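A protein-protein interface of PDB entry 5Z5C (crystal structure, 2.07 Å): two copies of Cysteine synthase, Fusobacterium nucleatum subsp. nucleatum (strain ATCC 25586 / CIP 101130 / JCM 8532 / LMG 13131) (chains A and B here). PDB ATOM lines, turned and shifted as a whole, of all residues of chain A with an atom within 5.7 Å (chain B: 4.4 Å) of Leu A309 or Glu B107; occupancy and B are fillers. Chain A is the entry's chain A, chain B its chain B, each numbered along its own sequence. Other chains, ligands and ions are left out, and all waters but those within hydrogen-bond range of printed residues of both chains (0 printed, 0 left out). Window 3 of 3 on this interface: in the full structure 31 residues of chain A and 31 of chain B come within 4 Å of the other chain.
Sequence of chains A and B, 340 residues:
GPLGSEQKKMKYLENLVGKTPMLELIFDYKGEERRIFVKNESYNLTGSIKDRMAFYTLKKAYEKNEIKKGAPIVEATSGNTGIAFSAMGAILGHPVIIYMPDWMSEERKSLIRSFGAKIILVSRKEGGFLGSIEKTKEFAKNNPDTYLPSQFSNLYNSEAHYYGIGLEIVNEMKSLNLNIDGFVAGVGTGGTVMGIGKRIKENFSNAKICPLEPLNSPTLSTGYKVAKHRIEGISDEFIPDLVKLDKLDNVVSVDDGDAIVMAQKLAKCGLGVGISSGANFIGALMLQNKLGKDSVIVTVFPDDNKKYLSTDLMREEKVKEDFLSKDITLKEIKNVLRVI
MLY A306 touches its own counterpart, MLY B306. MLY A306 touches MLY B307, but with the chains exchanged MLY A307 does not touch MLY B306 (4.1 Å). Of the 4 pairs that touch across the chains among the printed residues, 1 has its exchanged pair printed and touching as well.
NH1 of Arg B108 sits at hydrogen-bond distance from O of MLY B307 (3.1 Å). The backbone carbonyl oxygen (O) of Glu B107 sits at hydrogen-bond distance from the side-chain hydroxyl (OG) of Ser B110. The side-chain carboxylate (OE2) of Glu A107 sits at hydrogen-bond distance from the backbone NH (N) of Leu A309 (3.1 Å).
Hydrophobic or aromatic side chains of chain B within 4 Å of the printed part of chain A: Leu B111. Along chain B the printed residues that touch a printed residue of chain A span positions 107 to 307. Hydrophobic or aromatic side chains of chain A that line the printed part of chain B: Leu A309. Among the printed residues, no Asp or Glu carboxylate lies within 4 Å of a Lys or Arg side-chain nitrogen of the other chain.
Among the printed residues, pairs that only touch across the chains: MLY A306 with MLY B306 (3.8 Å), Asn A305 with Leu B111 (3.9 Å), Leu A309 with Glu B107 (3.9 Å) and MLY A306 with MLY B307 (3.9 Å).
Printed residues of chain B within 4 Å of MLY A306: MLY B306 (3.8 Å) and MLY B307 (3.9 Å). MLY A307 touches none of the printed residues of chain B. Glu B107 touches just one residue of chain A: Leu A309. Of the printed residues of chain A, MLY B306 touches MLY A306 (3.8 Å). Printed residues of chain A within 4 Å of MLY B307: MLY A306. The nearest printed residue of chain A that does not touch Glu B107 is MLY A306 (6.2 Å).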
ATOM      1  N   GLU A 107      -3.142  28.539  10.128  1.00  0.00           N
ATOM      2  CA  GLU A 107      -3.192  28.025   8.750  1.00  0.00           C
ATOM      3  C   GLU A 107      -4.636  27.846   8.287  1.00  0.00           C
ATOM      4  O   GLU A 107      -4.906  28.021   7.102  1.00  0.00           O
ATOM      5  CB  GLU A 107      -2.483  26.667   8.577  1.00  0.00           C
ATOM      6  CG  GLU A 107      -0.961  26.713   8.778  1.00  0.00           C
ATOM      7  CD  GLU A 107      -0.558  26.456  10.216  1.00  0.00           C
ATOM      8  OE1 GLU A 107      -1.334  26.828  11.135  1.00  0.00           O
ATOM      9  OE2 GLU A 107       0.512  25.836  10.414  1.00  0.00           O
ATOM     10  N   ASN A 305      -0.409  16.938   7.969  1.00  0.00           N
ATOM     11  CA  ASN A 305       0.259  17.728   9.012  1.00  0.00           C
ATOM     12  C   ASN A 305       0.480  19.213   8.621  1.00  0.00           C
ATOM     13  O   ASN A 305       0.923  19.979   9.475  1.00  0.00           O
ATOM     14  CB  ASN A 305       1.570  17.026   9.519  1.00  0.00           C
ATOM     15  CG  ASN A 305       2.598  16.793   8.423  1.00  0.00           C
ATOM     16  OD1 ASN A 305       2.322  16.918   7.198  1.00  0.00           O
ATOM     17  ND2 ASN A 305       3.808  16.475   8.850  1.00  0.00           N
ATOM     18  N   MLY A 306       0.132  19.651   7.394  1.00  0.00           N
ATOM     19  CA  MLY A 306       0.597  20.972   6.914  1.00  0.00           C
ATOM     20  CB  MLY A 306       0.380  21.122   5.411  1.00  0.00           C
ATOM     21  CG  MLY A 306       1.315  20.218   4.619  1.00  0.00           C
ATOM     22  CD  MLY A 306       1.292  20.582   3.138  1.00  0.00           C
ATOM     23  CE  MLY A 306       2.198  19.654   2.331  1.00  0.00           C
ATOM     24  NZ  MLY A 306       1.621  18.303   2.279  1.00  0.00           N
ATOM     25  C   MLY A 306      -0.140  22.081   7.606  1.00  0.00           C
ATOM     26  O   MLY A 306       0.393  23.159   7.712  1.00  0.00           O
ATOM     27  N   MLY A 307      -1.395  21.856   8.060  1.00  0.00           N
ATOM     28  CA  MLY A 307      -2.124  22.935   8.727  1.00  0.00           C
ATOM     29  CB  MLY A 307      -3.628  22.669   8.663  1.00  0.00           C
ATOM     30  CG  MLY A 307      -4.165  22.880   7.244  1.00  0.00           C
ATOM     31  CD  MLY A 307      -5.694  22.942   7.206  1.00  0.00           C
ATOM     32  CE  MLY A 307      -6.341  21.778   7.961  1.00  0.00           C
ATOM     33  NZ  MLY A 307      -6.146  20.514   7.232  1.00  0.00           N
ATOM     34  C   MLY A 307      -1.685  23.062  10.158  1.00  0.00           C
ATOM     35  O   MLY A 307      -2.257  23.890  10.869  1.00  0.00           O
ATOM     36  N   TYR A 308      -0.660  22.309  10.598  1.00  0.00           N
ATOM     37  CA  TYR A 308      -0.309  22.223  12.020  1.00  0.00           C
ATOM     38  C   TYR A 308       1.080  22.652  12.359  1.00  0.00           C
ATOM     39  O   TYR A 308       1.475  22.525  13.505  1.00  0.00           O
ATOM     40  CB  TYR A 308      -0.581  20.791  12.555  1.00  0.00           C
ATOM     41  CG  TYR A 308      -1.987  20.353  12.371  1.00  0.00           C
ATOM     42  CD1 TYR A 308      -2.389  19.728  11.199  1.00  0.00           C
ATOM     43  CD2 TYR A 308      -2.938  20.576  13.355  1.00  0.00           C
ATOM     44  CE1 TYR A 308      -3.684  19.323  11.017  1.00  0.00           C
ATOM     45  CE2 TYR A 308      -4.248  20.173  13.181  1.00  0.00           C
ATOM     46  CZ  TYR A 308      -4.614  19.547  12.005  1.00  0.00           C
ATOM     47  OH  TYR A 308      -5.914  19.142  11.800  1.00  0.00           O
ATOM     48  N   LEU A 309       1.799  23.230  11.394  1.00  0.00           N
ATOM     49  CA  LEU A 309       3.172  23.650  11.654  1.00  0.00           C
ATOM     50  C   LEU A 309       3.222  24.742  12.731  1.00  0.00           C
ATOM     51  O   LEU A 309       4.229  24.892  13.392  1.00  0.00           O
ATOM     52  CB  LEU A 309       3.906  24.157  10.397  1.00  0.00           C
ATOM     53  CG  LEU A 309       3.911  23.260   9.178  1.00  0.00           C
ATOM     54  CD1 LEU A 309       4.662  23.923   8.005  1.00  0.00           C
ATOM     55  CD2 LEU A 309       4.526  21.921   9.496  1.00  0.00           C
ATOM     56  N   SER A 310       2.160  25.525  12.883  1.00  0.00           N
ATOM     57  CA  SER A 310       2.154  26.565  13.918  1.00  0.00           C
ATOM     58  C   SER A 310       1.782  26.047  15.317  1.00  0.00           C
ATOM     59  O   SER A 310       1.710  26.875  16.242  1.00  0.00           O
ATOM     60  CB  SER A 310       1.145  27.682  13.524  1.00  0.00           C
ATOM     61  OG  SER A 310      -0.176  27.176  13.583  1.00  0.00           O
ATOM     62  N   THR A 311       1.486  24.742  15.449  1.00  0.00           N
ATOM     63  CA  THR A 311       0.850  24.197  16.626  1.00  0.00           C
ATOM     64  C   THR A 311       1.855  23.361  17.407  1.00  0.00           C
ATOM     65  O   THR A 311       3.039  23.213  16.998  1.00  0.00           O
ATOM     66  CB  THR A 311      -0.370  23.265  16.312  1.00  0.00           C
ATOM     67  OG1 THR A 311       0.076  22.028  15.752  1.00  0.00           O
ATOM     68  CG2 THR A 311      -1.389  23.908  15.400  1.00  0.00           C
ATOM     69  N   MET A 314       4.461  20.488  16.168  1.00  0.00           N
ATOM     70  CA  MET A 314       5.858  20.757  15.813  1.00  0.00           C
ATOM     71  C   MET A 314       6.766  21.048  17.003  1.00  0.00           C
ATOM     72  O   MET A 314       7.895  21.442  16.803  1.00  0.00           O
ATOM     73  CB  MET A 314       5.913  21.951  14.836  1.00  0.00           C
ATOM     74  CG  MET A 314       5.610  21.621  13.398  1.00  0.00           C
ATOM     75  SD  MET A 314       4.601  20.173  12.993  1.00  0.00           S
ATOM     76  CE  MET A 314       5.888  18.988  12.616  1.00  0.00           C
ATOM     77  N   ARG A 315       6.294  20.836  18.223  1.00  0.00           N
ATOM     78  CA  ARG A 315       7.033  21.157  19.439  1.00  0.00           C
ATOM     79  C   ARG A 315       7.211  19.863  20.207  1.00  0.00           C
ATOM     80  O   ARG A 315       6.664  18.831  19.822  1.00  0.00           O
ATOM     81  CB  ARG A 315       6.272  22.213  20.257  1.00  0.00           C
ATOM     82  CG  ARG A 315       6.079  23.522  19.526  1.00  0.00           C
ATOM     83  CD  ARG A 315       5.384  24.567  20.376  1.00  0.00           C
ATOM     84  NE  ARG A 315       5.229  25.819  19.630  1.00  0.00           N
ATOM     85  CZ  ARG A 315       4.065  26.282  19.136  1.00  0.00           C
ATOM     86  NH1 ARG A 315       2.921  25.654  19.398  1.00  0.00           N
ATOM     87  NH2 ARG A 315       4.043  27.410  18.438  1.00  0.00           N
ATOM     88  N   SER B 105      14.036  28.908   5.377  1.00  0.00           N
ATOM     89  CA  SER B 105      13.068  29.244   6.432  1.00  0.00           C
ATOM     90  C   SER B 105      12.758  28.079   7.368  1.00  0.00           C
ATOM     91  O   SER B 105      12.933  26.908   6.994  1.00  0.00           O
ATOM     92  CB  SER B 105      11.746  29.730   5.835  1.00  0.00           C
ATOM     93  OG  SER B 105      10.988  28.655   5.307  1.00  0.00           O
ATOM     94  N   GLU B 106      12.264  28.440   8.557  1.00  0.00           N
ATOM     95  CA  GLU B 106      11.880  27.503   9.626  1.00  0.00           C
ATOM     96  C   GLU B 106      10.794  26.538   9.099  1.00  0.00           C
ATOM     97  O   GLU B 106      10.881  25.334   9.299  1.00  0.00           O
ATOM     98  CB  GLU B 106      11.453  28.272  10.917  1.00  0.00           C
ATOM     99  CG  GLU B 106       9.940  28.410  11.289  1.00  0.00           C
ATOM    100  CD  GLU B 106       9.099  29.402  10.485  1.00  0.00           C
ATOM    101  OE1 GLU B 106       9.532  29.827   9.386  1.00  0.00           O
ATOM    102  OE2 GLU B 106       7.981  29.733  10.943  1.00  0.00           O
ATOM    103  N   GLU B 107       9.813  27.096   8.382  1.00  0.00           N
ATOM    104  CA  GLU B 107       8.700  26.347   7.835  1.00  0.00           C
ATOM    105  C   GLU B 107       9.153  25.150   6.981  1.00  0.00           C
ATOM    106  O   GLU B 107       8.650  24.056   7.169  1.00  0.00           O
ATOM    107  CB  GLU B 107       7.723  27.299   7.082  1.00  0.00           C
ATOM    108  CG  GLU B 107       6.804  26.605   6.094  1.00  0.00           C
ATOM    109  CD  GLU B 107       5.626  27.430   5.599  1.00  0.00           C
ATOM    110  OE1 GLU B 107       5.661  28.673   5.732  1.00  0.00           O
ATOM    111  OE2 GLU B 107       4.676  26.828   5.058  1.00  0.00           O
ATOM    112  N   ARG B 108      10.124  25.345   6.098  1.00  0.00           N
ATOM    113  CA  ARG B 108      10.624  24.243   5.235  1.00  0.00           C
ATOM    114  C   ARG B 108      11.323  23.160   6.056  1.00  0.00           C
ATOM    115  O   ARG B 108      11.156  21.958   5.791  1.00  0.00           O
ATOM    116  CB  ARG B 108      11.642  24.674   4.177  1.00  0.00           C
ATOM    117  CG  ARG B 108      11.444  26.074   3.629  1.00  0.00           C
ATOM    118  CD  ARG B 108      10.015  26.327   3.213  1.00  0.00           C
ATOM    119  NE  ARG B 108       9.643  25.537   2.046  1.00  0.00           N
ATOM    120  CZ  ARG B 108       8.465  25.613   1.435  1.00  0.00           C
ATOM    121  NH1 ARG B 108       7.516  26.411   1.909  1.00  0.00           N
ATOM    122  NH2 ARG B 108       8.227  24.868   0.369  1.00  0.00           N
ATOM    123  N   MLY B 109      12.137  23.615   7.019  1.00  0.00           N
ATOM    124  CA  MLY B 109      12.969  22.720   7.837  1.00  0.00           C
ATOM    125  CB  MLY B 109      13.933  23.529   8.710  1.00  0.00           C
ATOM    126  CG  MLY B 109      15.031  24.190   7.875  1.00  0.00           C
ATOM    127  CD  MLY B 109      16.112  24.842   8.747  1.00  0.00           C
ATOM    128  CE  MLY B 109      15.636  26.170   9.342  1.00  0.00           C
ATOM    129  NZ  MLY B 109      16.672  26.775  10.201  1.00  0.00           N
ATOM    130  CH1 MLY B 109      17.670  27.493   9.387  1.00  0.00           C
ATOM    131  CH2 MLY B 109      16.042  27.708  11.152  1.00  0.00           C
ATOM    132  C   MLY B 109      12.066  21.869   8.686  1.00  0.00           C
ATOM    133  O   MLY B 109      12.189  20.628   8.663  1.00  0.00           O
ATOM    134  N   SER B 110      11.090  22.507   9.364  1.00  0.00           N
ATOM    135  CA  SER B 110      10.138  21.780  10.230  1.00  0.00           C
ATOM    136  C   SER B 110       9.338  20.725   9.476  1.00  0.00           C
ATOM    137  O   SER B 110       9.155  19.623   9.971  1.00  0.00           O
ATOM    138  CB  SER B 110       9.208  22.721  11.019  1.00  0.00           C
ATOM    139  OG  SER B 110       8.335  23.441  10.165  1.00  0.00           O
ATOM    140  N   LEU B 111       8.874  21.031   8.265  1.00  0.00           N
ATOM    141  CA  LEU B 111       8.087  20.040   7.527  1.00  0.00           C
ATOM    142  C   LEU B 111       8.965  18.809   7.167  1.00  0.00           C
ATOM    143  O   LEU B 111       8.596  17.654   7.367  1.00  0.00           O
ATOM    144  CB  LEU B 111       7.474  20.658   6.266  1.00  0.00           C
ATOM    145  CG  LEU B 111       6.449  19.825   5.485  1.00  0.00           C
ATOM    146  CD1 LEU B 111       5.468  19.125   6.412  1.00  0.00           C
ATOM    147  CD2 LEU B 111       5.715  20.713   4.475  1.00  0.00           C
ATOM    148  N   MLY B 306      -0.855  25.003   0.655  1.00  0.00           N
ATOM    149  CA  MLY B 306      -0.699  24.982   2.134  1.00  0.00           C
ATOM    150  CB  MLY B 306      -1.048  23.610   2.724  1.00  0.00           C
ATOM    151  CG  MLY B 306      -2.539  23.296   2.606  1.00  0.00           C
ATOM    152  CD  MLY B 306      -2.889  22.021   3.373  1.00  0.00           C
ATOM    153  CE  MLY B 306      -4.375  21.681   3.282  1.00  0.00           C
ATOM    154  NZ  MLY B 306      -4.778  21.479   1.886  1.00  0.00           N
ATOM    155  C   MLY B 306       0.709  25.334   2.540  1.00  0.00           C
ATOM    156  O   MLY B 306       0.854  25.836   3.622  1.00  0.00           O
ATOM    157  N   MLY B 307       1.760  25.109   1.730  1.00  0.00           N
ATOM    158  CA  MLY B 307       3.132  25.489   2.164  1.00  0.00           C
ATOM    159  CB  MLY B 307       4.181  24.608   1.495  1.00  0.00           C
ATOM    160  CG  MLY B 307       4.027  23.139   1.880  1.00  0.00           C
ATOM    161  CD  MLY B 307       5.144  22.287   1.278  1.00  0.00           C
ATOM    162  CE  MLY B 307       5.234  22.449  -0.246  1.00  0.00           C
ATOM    163  NZ  MLY B 307       4.031  21.894  -0.899  1.00  0.00           N
ATOM    164  C   MLY B 307       3.440  26.918   1.817  1.00  0.00           C
ATOM    165  O   MLY B 307       4.567  27.334   2.003  1.00  0.00           O
ATOM    166  N   SER B 310       2.664  32.060   4.018  1.00  0.00           N
ATOM    167  CA  SER B 310       3.286  33.311   4.386  1.00  0.00           C
ATOM    168  C   SER B 310       4.066  33.898   3.215  1.00  0.00           C
ATOM    169  O   SER B 310       4.896  34.770   3.427  1.00  0.00           O
ATOM    170  CB  SER B 310       4.174  33.075   5.591  1.00  0.00           C
ATOM    171  OG  SER B 310       5.266  32.273   5.177  1.00  0.00           O
